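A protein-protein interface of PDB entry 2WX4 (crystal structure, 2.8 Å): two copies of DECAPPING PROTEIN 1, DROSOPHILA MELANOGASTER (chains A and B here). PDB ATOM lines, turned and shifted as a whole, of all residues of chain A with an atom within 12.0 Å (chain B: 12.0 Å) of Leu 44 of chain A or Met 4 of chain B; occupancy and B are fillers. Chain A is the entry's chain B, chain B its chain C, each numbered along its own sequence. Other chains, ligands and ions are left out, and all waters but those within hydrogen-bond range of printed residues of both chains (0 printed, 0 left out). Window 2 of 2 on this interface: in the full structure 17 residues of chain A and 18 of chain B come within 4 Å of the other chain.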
ATOM      1  N   HIS A  33      -0.719  11.582  -6.377  1.00  0.00           N
ATOM      2  CA  HIS A  33      -1.365  10.283  -6.483  1.00  0.00           C
ATOM      3  C   HIS A  33      -1.193   9.682  -7.876  1.00  0.00           C
ATOM      4  O   HIS A  33      -0.960   8.488  -8.008  1.00  0.00           O
ATOM      5  CB  HIS A  33      -2.837  10.380  -6.102  1.00  0.00           C
ATOM      6  CG  HIS A  33      -3.534   9.055  -6.046  1.00  0.00           C
ATOM      7  ND1 HIS A  33      -4.653   8.774  -6.795  1.00  0.00           N
ATOM      8  CD2 HIS A  33      -3.263   7.931  -5.339  1.00  0.00           C
ATOM      9  CE1 HIS A  33      -5.043   7.535  -6.548  1.00  0.00           C
ATOM     10  NE2 HIS A  33      -4.215   7.001  -5.671  1.00  0.00           N
ATOM     11  N   LYS A  34      -1.299  10.521  -8.904  1.00  0.00           N
ATOM     12  CA  LYS A  34      -1.027  10.117 -10.288  1.00  0.00           C
ATOM     13  C   LYS A  34       0.434   9.667 -10.463  1.00  0.00           C
ATOM     14  O   LYS A  34       0.683   8.578 -10.985  1.00  0.00           O
ATOM     15  CB  LYS A  34      -1.420  11.232 -11.271  1.00  0.00           C
ATOM     16  CG  LYS A  34      -1.396  10.839 -12.748  1.00  0.00           C
ATOM     17  CD  LYS A  34      -1.956  11.974 -13.657  1.00  0.00           C
ATOM     18  CE  LYS A  34      -1.976  11.562 -15.156  1.00  0.00           C
ATOM     19  NZ  LYS A  34      -2.945  12.322 -16.007  1.00  0.00           N
ATOM     20  N   ALA A  35       1.387  10.484 -10.004  1.00  0.00           N
ATOM     21  CA  ALA A  35       2.783  10.053  -9.895  1.00  0.00           C
ATOM     22  C   ALA A  35       2.850   8.621  -9.379  1.00  0.00           C
ATOM     23  O   ALA A  35       3.419   7.753 -10.032  1.00  0.00           O
ATOM     24  CB  ALA A  35       3.582  10.979  -8.990  1.00  0.00           C
ATOM     25  N   TYR A  36       2.239   8.390  -8.218  1.00  0.00           N
ATOM     26  CA  TYR A  36       2.186   7.080  -7.560  1.00  0.00           C
ATOM     27  C   TYR A  36       1.573   5.967  -8.417  1.00  0.00           C
ATOM     28  O   TYR A  36       2.131   4.889  -8.517  1.00  0.00           O
ATOM     29  CB  TYR A  36       1.429   7.203  -6.229  1.00  0.00           C
ATOM     30  CG  TYR A  36       0.953   5.896  -5.640  1.00  0.00           C
ATOM     31  CD1 TYR A  36       1.833   5.035  -5.000  1.00  0.00           C
ATOM     32  CD2 TYR A  36      -0.389   5.518  -5.722  1.00  0.00           C
ATOM     33  CE1 TYR A  36       1.383   3.818  -4.463  1.00  0.00           C
ATOM     34  CE2 TYR A  36      -0.848   4.293  -5.184  1.00  0.00           C
ATOM     35  CZ  TYR A  36       0.040   3.459  -4.561  1.00  0.00           C
ATOM     36  OH  TYR A  36      -0.401   2.275  -4.018  1.00  0.00           O
ATOM     37  N   LEU A  37       0.417   6.229  -9.018  1.00  0.00           N
ATOM     38  CA  LEU A  37      -0.222   5.266  -9.919  1.00  0.00           C
ATOM     39  C   LEU A  37       0.677   4.897 -11.078  1.00  0.00           C
ATOM     40  O   LEU A  37       0.794   3.723 -11.437  1.00  0.00           O
ATOM     41  CB  LEU A  37      -1.541   5.813 -10.455  1.00  0.00           C
ATOM     42  CG  LEU A  37      -2.623   5.785  -9.383  1.00  0.00           C
ATOM     43  CD1 LEU A  37      -3.940   6.254  -9.937  1.00  0.00           C
ATOM     44  CD2 LEU A  37      -2.757   4.401  -8.764  1.00  0.00           C
ATOM     45  N   ASN A  38       1.309   5.910 -11.663  1.00  0.00           N
ATOM     46  CA  ASN A  38       2.220   5.681 -12.759  1.00  0.00           C
ATOM     47  C   ASN A  38       3.388   4.781 -12.361  1.00  0.00           C
ATOM     48  O   ASN A  38       3.772   3.896 -13.112  1.00  0.00           O
ATOM     49  CB  ASN A  38       2.711   6.991 -13.350  1.00  0.00           C
ATOM     50  CG  ASN A  38       3.350   6.788 -14.706  1.00  0.00           C
ATOM     51  OD1 ASN A  38       2.658   6.568 -15.712  1.00  0.00           O
ATOM     52  ND2 ASN A  38       4.688   6.817 -14.742  1.00  0.00           N
ATOM     53  N   GLY A  39       3.931   5.002 -11.167  1.00  0.00           N
ATOM     54  CA  GLY A  39       4.977   4.156 -10.630  1.00  0.00           C
ATOM     55  C   GLY A  39       4.468   2.746 -10.472  1.00  0.00           C
ATOM     56  O   GLY A  39       5.122   1.795 -10.910  1.00  0.00           O
ATOM     57  N   CYS A  40       3.293   2.622  -9.853  1.00  0.00           N
ATOM     58  CA  CYS A  40       2.586   1.346  -9.678  1.00  0.00           C
ATOM     59  C   CYS A  40       2.398   0.592 -10.984  1.00  0.00           C
ATOM     60  O   CYS A  40       2.628  -0.625 -11.040  1.00  0.00           O
ATOM     61  CB  CYS A  40       1.220   1.578  -9.034  1.00  0.00           C
ATOM     62  SG  CYS A  40       1.274   1.735  -7.247  1.00  0.00           S
ATOM     63  N   SER A  41       1.994   1.321 -12.027  1.00  0.00           N
ATOM     64  CA  SER A  41       1.760   0.728 -13.328  1.00  0.00           C
ATOM     65  C   SER A  41       3.022   0.071 -13.858  1.00  0.00           C
ATOM     66  O   SER A  41       2.985  -1.097 -14.254  1.00  0.00           O
ATOM     67  CB  SER A  41       1.222   1.755 -14.328  1.00  0.00           C
ATOM     68  OG  SER A  41       0.644   1.110 -15.462  1.00  0.00           O
ATOM     69  N   ASN A  42       4.133   0.812 -13.829  1.00  0.00           N
ATOM     70  CA  ASN A  42       5.419   0.295 -14.291  1.00  0.00           C
ATOM     71  C   ASN A  42       5.762  -0.980 -13.540  1.00  0.00           C
ATOM     72  O   ASN A  42       6.099  -1.998 -14.141  1.00  0.00           O
ATOM     73  CB  ASN A  42       6.548   1.321 -14.110  1.00  0.00           C
ATOM     74  CG  ASN A  42       6.344   2.603 -14.939  1.00  0.00           C
ATOM     75  OD1 ASN A  42       5.619   2.618 -15.943  1.00  0.00           O
ATOM     76  ND2 ASN A  42       6.990   3.691 -14.506  1.00  0.00           N
ATOM     77  N   LEU A  43       5.646  -0.922 -12.221  1.00  0.00           N
ATOM     78  CA  LEU A  43       5.973  -2.055 -11.391  1.00  0.00           C
ATOM     79  C   LEU A  43       5.120  -3.276 -11.680  1.00  0.00           C
ATOM     80  O   LEU A  43       5.662  -4.372 -11.894  1.00  0.00           O
ATOM     81  CB  LEU A  43       5.863  -1.682  -9.917  1.00  0.00           C
ATOM     82  CG  LEU A  43       7.214  -1.394  -9.283  1.00  0.00           C
ATOM     83  CD1 LEU A  43       7.051  -0.744  -7.928  1.00  0.00           C
ATOM     84  CD2 LEU A  43       8.008  -2.685  -9.186  1.00  0.00           C
ATOM     85  N   LEU A  44       3.799  -3.084 -11.703  1.00  0.00           N
ATOM     86  CA  LEU A  44       2.860  -4.205 -11.743  1.00  0.00           C
ATOM     87  C   LEU A  44       2.631  -4.740 -13.132  1.00  0.00           C
ATOM     88  O   LEU A  44       2.541  -5.943 -13.325  1.00  0.00           O
ATOM     89  CB  LEU A  44       1.516  -3.837 -11.106  1.00  0.00           C
ATOM     90  CG  LEU A  44       1.517  -3.503  -9.611  1.00  0.00           C
ATOM     91  CD1 LEU A  44       0.204  -2.895  -9.214  1.00  0.00           C
ATOM     92  CD2 LEU A  44       1.813  -4.705  -8.763  1.00  0.00           C
ATOM     93  N   LEU A  45       2.532  -3.851 -14.105  1.00  0.00           N
ATOM     94  CA  LEU A  45       2.280  -4.276 -15.472  1.00  0.00           C
ATOM     95  C   LEU A  45       3.616  -4.380 -16.202  1.00  0.00           C
ATOM     96  O   LEU A  45       3.671  -4.600 -17.412  1.00  0.00           O
ATOM     97  CB  LEU A  45       1.292  -3.322 -16.138  1.00  0.00           C
ATOM     98  CG  LEU A  45       0.101  -3.028 -15.220  1.00  0.00           C
ATOM     99  CD1 LEU A  45      -0.704  -1.855 -15.701  1.00  0.00           C
ATOM    100  CD2 LEU A  45      -0.785  -4.221 -15.029  1.00  0.00           C
ATOM    101  N   ASP A  46       4.685  -4.242 -15.410  1.00  0.00           N
ATOM    102  CA  ASP A  46       6.103  -4.408 -15.810  1.00  0.00           C
ATOM    103  C   ASP A  46       6.561  -3.508 -16.979  1.00  0.00           C
ATOM    104  O   ASP A  46       5.998  -2.427 -17.252  1.00  0.00           O
ATOM    105  CB  ASP A  46       6.486  -5.896 -16.018  1.00  0.00           C
ATOM    106  CG  ASP A  46       6.679  -6.667 -14.686  1.00  0.00           C
ATOM    107  OD1 ASP A  46       5.760  -6.676 -13.825  1.00  0.00           O
ATOM    108  OD2 ASP A  46       7.756  -7.293 -14.512  1.00  0.00           O
ATOM    109  OXT ASP A  46       7.530  -3.861 -17.672  1.00  0.00           O
ATOM    110  N   GLY B   1       3.644 -15.321  -3.646  1.00  0.00           N
ATOM    111  CA  GLY B   1       3.146 -14.318  -2.659  1.00  0.00           C
ATOM    112  C   GLY B   1       1.671 -14.033  -2.883  1.00  0.00           C
ATOM    113  O   GLY B   1       0.932 -14.911  -3.372  1.00  0.00           O
ATOM    114  N   PRO B   2       1.222 -12.817  -2.495  1.00  0.00           N
ATOM    115  CA  PRO B   2      -0.131 -12.300  -2.721  1.00  0.00           C
ATOM    116  C   PRO B   2      -0.215 -11.508  -4.014  1.00  0.00           C
ATOM    117  O   PRO B   2       0.805 -11.299  -4.672  1.00  0.00           O
ATOM    118  CB  PRO B   2      -0.339 -11.366  -1.528  1.00  0.00           C
ATOM    119  CG  PRO B   2       1.015 -10.832  -1.258  1.00  0.00           C
ATOM    120  CD  PRO B   2       1.932 -12.015  -1.466  1.00  0.00           C
ATOM    121  N   HIS B   3      -1.417 -11.050  -4.348  1.00  0.00           N
ATOM    122  CA  HIS B   3      -1.673 -10.379  -5.609  1.00  0.00           C
ATOM    123  C   HIS B   3      -1.391  -8.898  -5.402  1.00  0.00           C
ATOM    124  O   HIS B   3      -2.224  -8.162  -4.912  1.00  0.00           O
ATOM    125  CB  HIS B   3      -3.107 -10.690  -6.059  1.00  0.00           C
ATOM    126  CG  HIS B   3      -3.514 -10.048  -7.345  1.00  0.00           C
ATOM    127  ND1 HIS B   3      -2.867 -10.281  -8.538  1.00  0.00           N
ATOM    128  CD2 HIS B   3      -4.538  -9.213  -7.633  1.00  0.00           C
ATOM    129  CE1 HIS B   3      -3.450  -9.588  -9.498  1.00  0.00           C
ATOM    130  NE2 HIS B   3      -4.469  -8.934  -8.975  1.00  0.00           N
ATOM    131  N   MET B   4      -0.178  -8.503  -5.788  1.00  0.00           N
ATOM    132  CA  MET B   4       0.407  -7.183  -5.544  1.00  0.00           C
ATOM    133  C   MET B   4      -0.492  -6.027  -5.905  1.00  0.00           C
ATOM    134  O   MET B   4      -0.565  -5.043  -5.175  1.00  0.00           O
ATOM    135  CB  MET B   4       1.696  -7.035  -6.342  1.00  0.00           C
ATOM    136  CG  MET B   4       2.844  -7.912  -5.904  1.00  0.00           C
ATOM    137  SD  MET B   4       3.165  -7.540  -4.189  1.00  0.00           S
ATOM    138  CE  MET B   4       3.322  -9.186  -3.489  1.00  0.00           C
ATOM    139  N   ALA B   5      -1.161  -6.138  -7.047  1.00  0.00           N
ATOM    140  CA  ALA B   5      -2.081  -5.118  -7.514  1.00  0.00           C
ATOM    141  C   ALA B   5      -3.070  -4.687  -6.440  1.00  0.00           C
ATOM    142  O   ALA B   5      -3.445  -3.521  -6.393  1.00  0.00           O
ATOM    143  CB  ALA B   5      -2.809  -5.612  -8.718  1.00  0.00           C
ATOM    144  N   ASP B   6      -3.486  -5.623  -5.587  1.00  0.00           N
ATOM    145  CA  ASP B   6      -4.406  -5.348  -4.483  1.00  0.00           C
ATOM    146  C   ASP B   6      -3.843  -4.454  -3.380  1.00  0.00           C
ATOM    147  O   ASP B   6      -4.528  -4.182  -2.387  1.00  0.00           O
ATOM    148  CB  ASP B   6      -4.910  -6.664  -3.872  1.00  0.00           C
ATOM    149  CG  ASP B   6      -5.911  -7.390  -4.771  1.00  0.00           C
ATOM    150  OD1 ASP B   6      -6.472  -6.767  -5.698  1.00  0.00           O
ATOM    151  OD2 ASP B   6      -6.151  -8.597  -4.550  1.00  0.00           O
ATOM    152  N   LEU B   7      -2.604  -3.997  -3.535  1.00  0.00           N
ATOM    153  CA  LEU B   7      -2.022  -3.056  -2.566  1.00  0.00           C
ATOM    154  C   LEU B   7      -2.324  -1.619  -2.964  1.00  0.00           C
ATOM    155  O   LEU B   7      -2.219  -0.695  -2.158  1.00  0.00           O
ATOM    156  CB  LEU B   7      -0.523  -3.262  -2.415  1.00  0.00           C
ATOM    157  CG  LEU B   7      -0.104  -4.633  -1.891  1.00  0.00           C
ATOM    158  CD1 LEU B   7       1.387  -4.862  -2.156  1.00  0.00           C
ATOM    159  CD2 LEU B   7      -0.439  -4.808  -0.408  1.00  0.00           C
ATOM    160  N   LEU B   8      -2.718  -1.451  -4.216  1.00  0.00           N
ATOM    161  CA  LEU B   8      -3.029  -0.167  -4.784  1.00  0.00           C
ATOM    162  C   LEU B   8      -3.894   0.685  -3.846  1.00  0.00           C
ATOM    163  O   LEU B   8      -5.014   0.297  -3.526  1.00  0.00           O
ATOM    164  CB  LEU B   8      -3.764  -0.414  -6.091  1.00  0.00           C
ATOM    165  CG  LEU B   8      -3.445   0.403  -7.334  1.00  0.00           C
ATOM    166  CD1 LEU B   8      -1.980   0.766  -7.417  1.00  0.00           C
ATOM    167  CD2 LEU B   8      -3.837  -0.460  -8.515  1.00  0.00           C
ATOM    168  N   LEU B   9      -3.352   1.829  -3.418  1.00  0.00           N
ATOM    169  CA  LEU B   9      -4.034   2.780  -2.539  1.00  0.00           C
ATOM    170  C   LEU B   9      -4.918   3.765  -3.298  1.00  0.00           C
ATOM    171  O   LEU B   9      -4.489   4.349  -4.279  1.00  0.00           O
ATOM    172  CB  LEU B   9      -3.009   3.583  -1.722  1.00  0.00           C
ATOM    173  CG  LEU B   9      -2.077   2.882  -0.722  1.00  0.00           C
ATOM    174  CD1 LEU B   9      -1.391   3.907   0.150  1.00  0.00           C
ATOM    175  CD2 LEU B   9      -2.811   1.856   0.154  1.00  0.00           C
ATOM    176  N   ASN B  10      -6.146   3.965  -2.835  1.00  0.00           N
ATOM    177  CA  ASN B  10      -6.985   5.010  -3.389  1.00  0.00           C
ATOM    178  C   ASN B  10      -6.491   6.356  -2.879  1.00  0.00           C
ATOM    179  O   ASN B  10      -5.713   6.410  -1.933  1.00  0.00           O
ATOM    180  CB  ASN B  10      -8.464   4.775  -3.052  1.00  0.00           C
ATOM    181  CG  ASN B  10      -8.800   5.015  -1.582  1.00  0.00           C
ATOM    182  OD1 ASN B  10      -8.428   6.034  -0.988  1.00  0.00           O
ATOM    183  ND2 ASN B  10      -9.544   4.088  -1.002  1.00  0.00           N
ATOM    184  N   GLN B  13      -6.590   6.863   0.991  1.00  0.00           N
ATOM    185  CA  GLN B  13      -5.614   6.039   1.697  1.00  0.00           C
ATOM    186  C   GLN B  13      -4.198   6.518   1.422  1.00  0.00           C
ATOM    187  O   GLN B  13      -3.329   6.483   2.286  1.00  0.00           O
ATOM    188  CB  GLN B  13      -5.724   4.596   1.268  1.00  0.00           C
ATOM    189  CG  GLN B  13      -7.087   4.045   1.432  1.00  0.00           C
ATOM    190  CD  GLN B  13      -7.207   2.675   0.849  1.00  0.00           C
ATOM    191  OE1 GLN B  13      -6.954   2.468  -0.335  1.00  0.00           O
ATOM    192  NE2 GLN B  13      -7.586   1.717   1.674  1.00  0.00           N
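The side-chain hydroxyl (OH) of Tyr 36 of chain A lies within hydrogen-bond range of the backbone NH (N) of Leu 9 of chain B (3.0 Å). A ring nitrogen (NE2) of His 33 of chain A sits at hydrogen-bond distance from the backbone carbonyl oxygen of Leu 9 of chain B (3.0 Å).
The backbone NH of Gln 13 of chain B lies within hydrogen-bond range of the side-chain amide oxygen of Asn 10 of chain B, 2.8 Å away. O of Tyr 36 of chain A lies close to SG of Cys 40 of chain A, at 3.5 Å.
Among the printed residues, merely in contact across the chains: Leu 44 of chain A with Met 4 of chain B, Cys 40 of chain A with Leu 8 of chain B, Leu 44 of chain A with Ala 5 of chain B, His 33 of chain A with Asn 10 of chain B, Tyr 36 of chain A with Leu 8 of chain B, Tyr 36 of chain A with Leu 7 of chain B and Leu 37 of chain A with Leu 8 of chain B.
Lys 34 of chain A touches none of the printed residues of chain B. Of the printed residues of chain B, Tyr 36 of chain A touches Leu 7, Leu 8 and Leu 9. Printed residues of chain B within 4 Å of Leu 37 of chain A: Leu 8. Cys 40 of chain A touches just one residue of chain B: Leu 8. No residue of chain B comes within 4 Å of Ser 41 of chain A. Leu 43 of chain A touches none of the printed residues of chain B. Leu 44 of chain A touches just these residues of chain B: Met 4 and Ala 5. No residue of chain B comes within 4 Å of Asp 46 of chain A. No residue of chain A comes within 4 Å of Gly 1 of chain B. No residue of chain A comes within 4 Å of Pro 2 of chain B. Of the printed residues of chain A, Met 4 of chain B touches Leu 44. Of the printed residues of chain A, Leu 7 of chain B touches Tyr 36. Printed residues of chain A within 4 Å of Leu 9 of chain B: His 33 and Tyr 36. Printed residues of chain A within 4 Å of Asn 10 of chain B: His 33 (3.7 Å). The nearest residue of chain B that does not touch Leu 44 of chain A is Leu 8 of chain B (4.6 Å). The nearest printed residue of chain A that does not touch Leu 9 of chain B is Leu 37 of chain A (4.8 Å).
Of the 14 printed residues of chain A, 5 touch a printed residue of chain B. Along chain A the printed residues that touch a printed residue of chain B span positions 33 to 44. Among the printed residues, 9 pairs touch across the chains. Among the printed residues, no Asp or Glu carboxylate lies within 4 Å of a Lys or Arg side-chain nitrogen of the other chain.
No position is printed for both chains. Of the 9 pairs that touch across the chains among the printed residues, none has its exchanged pair printed and touching as well.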
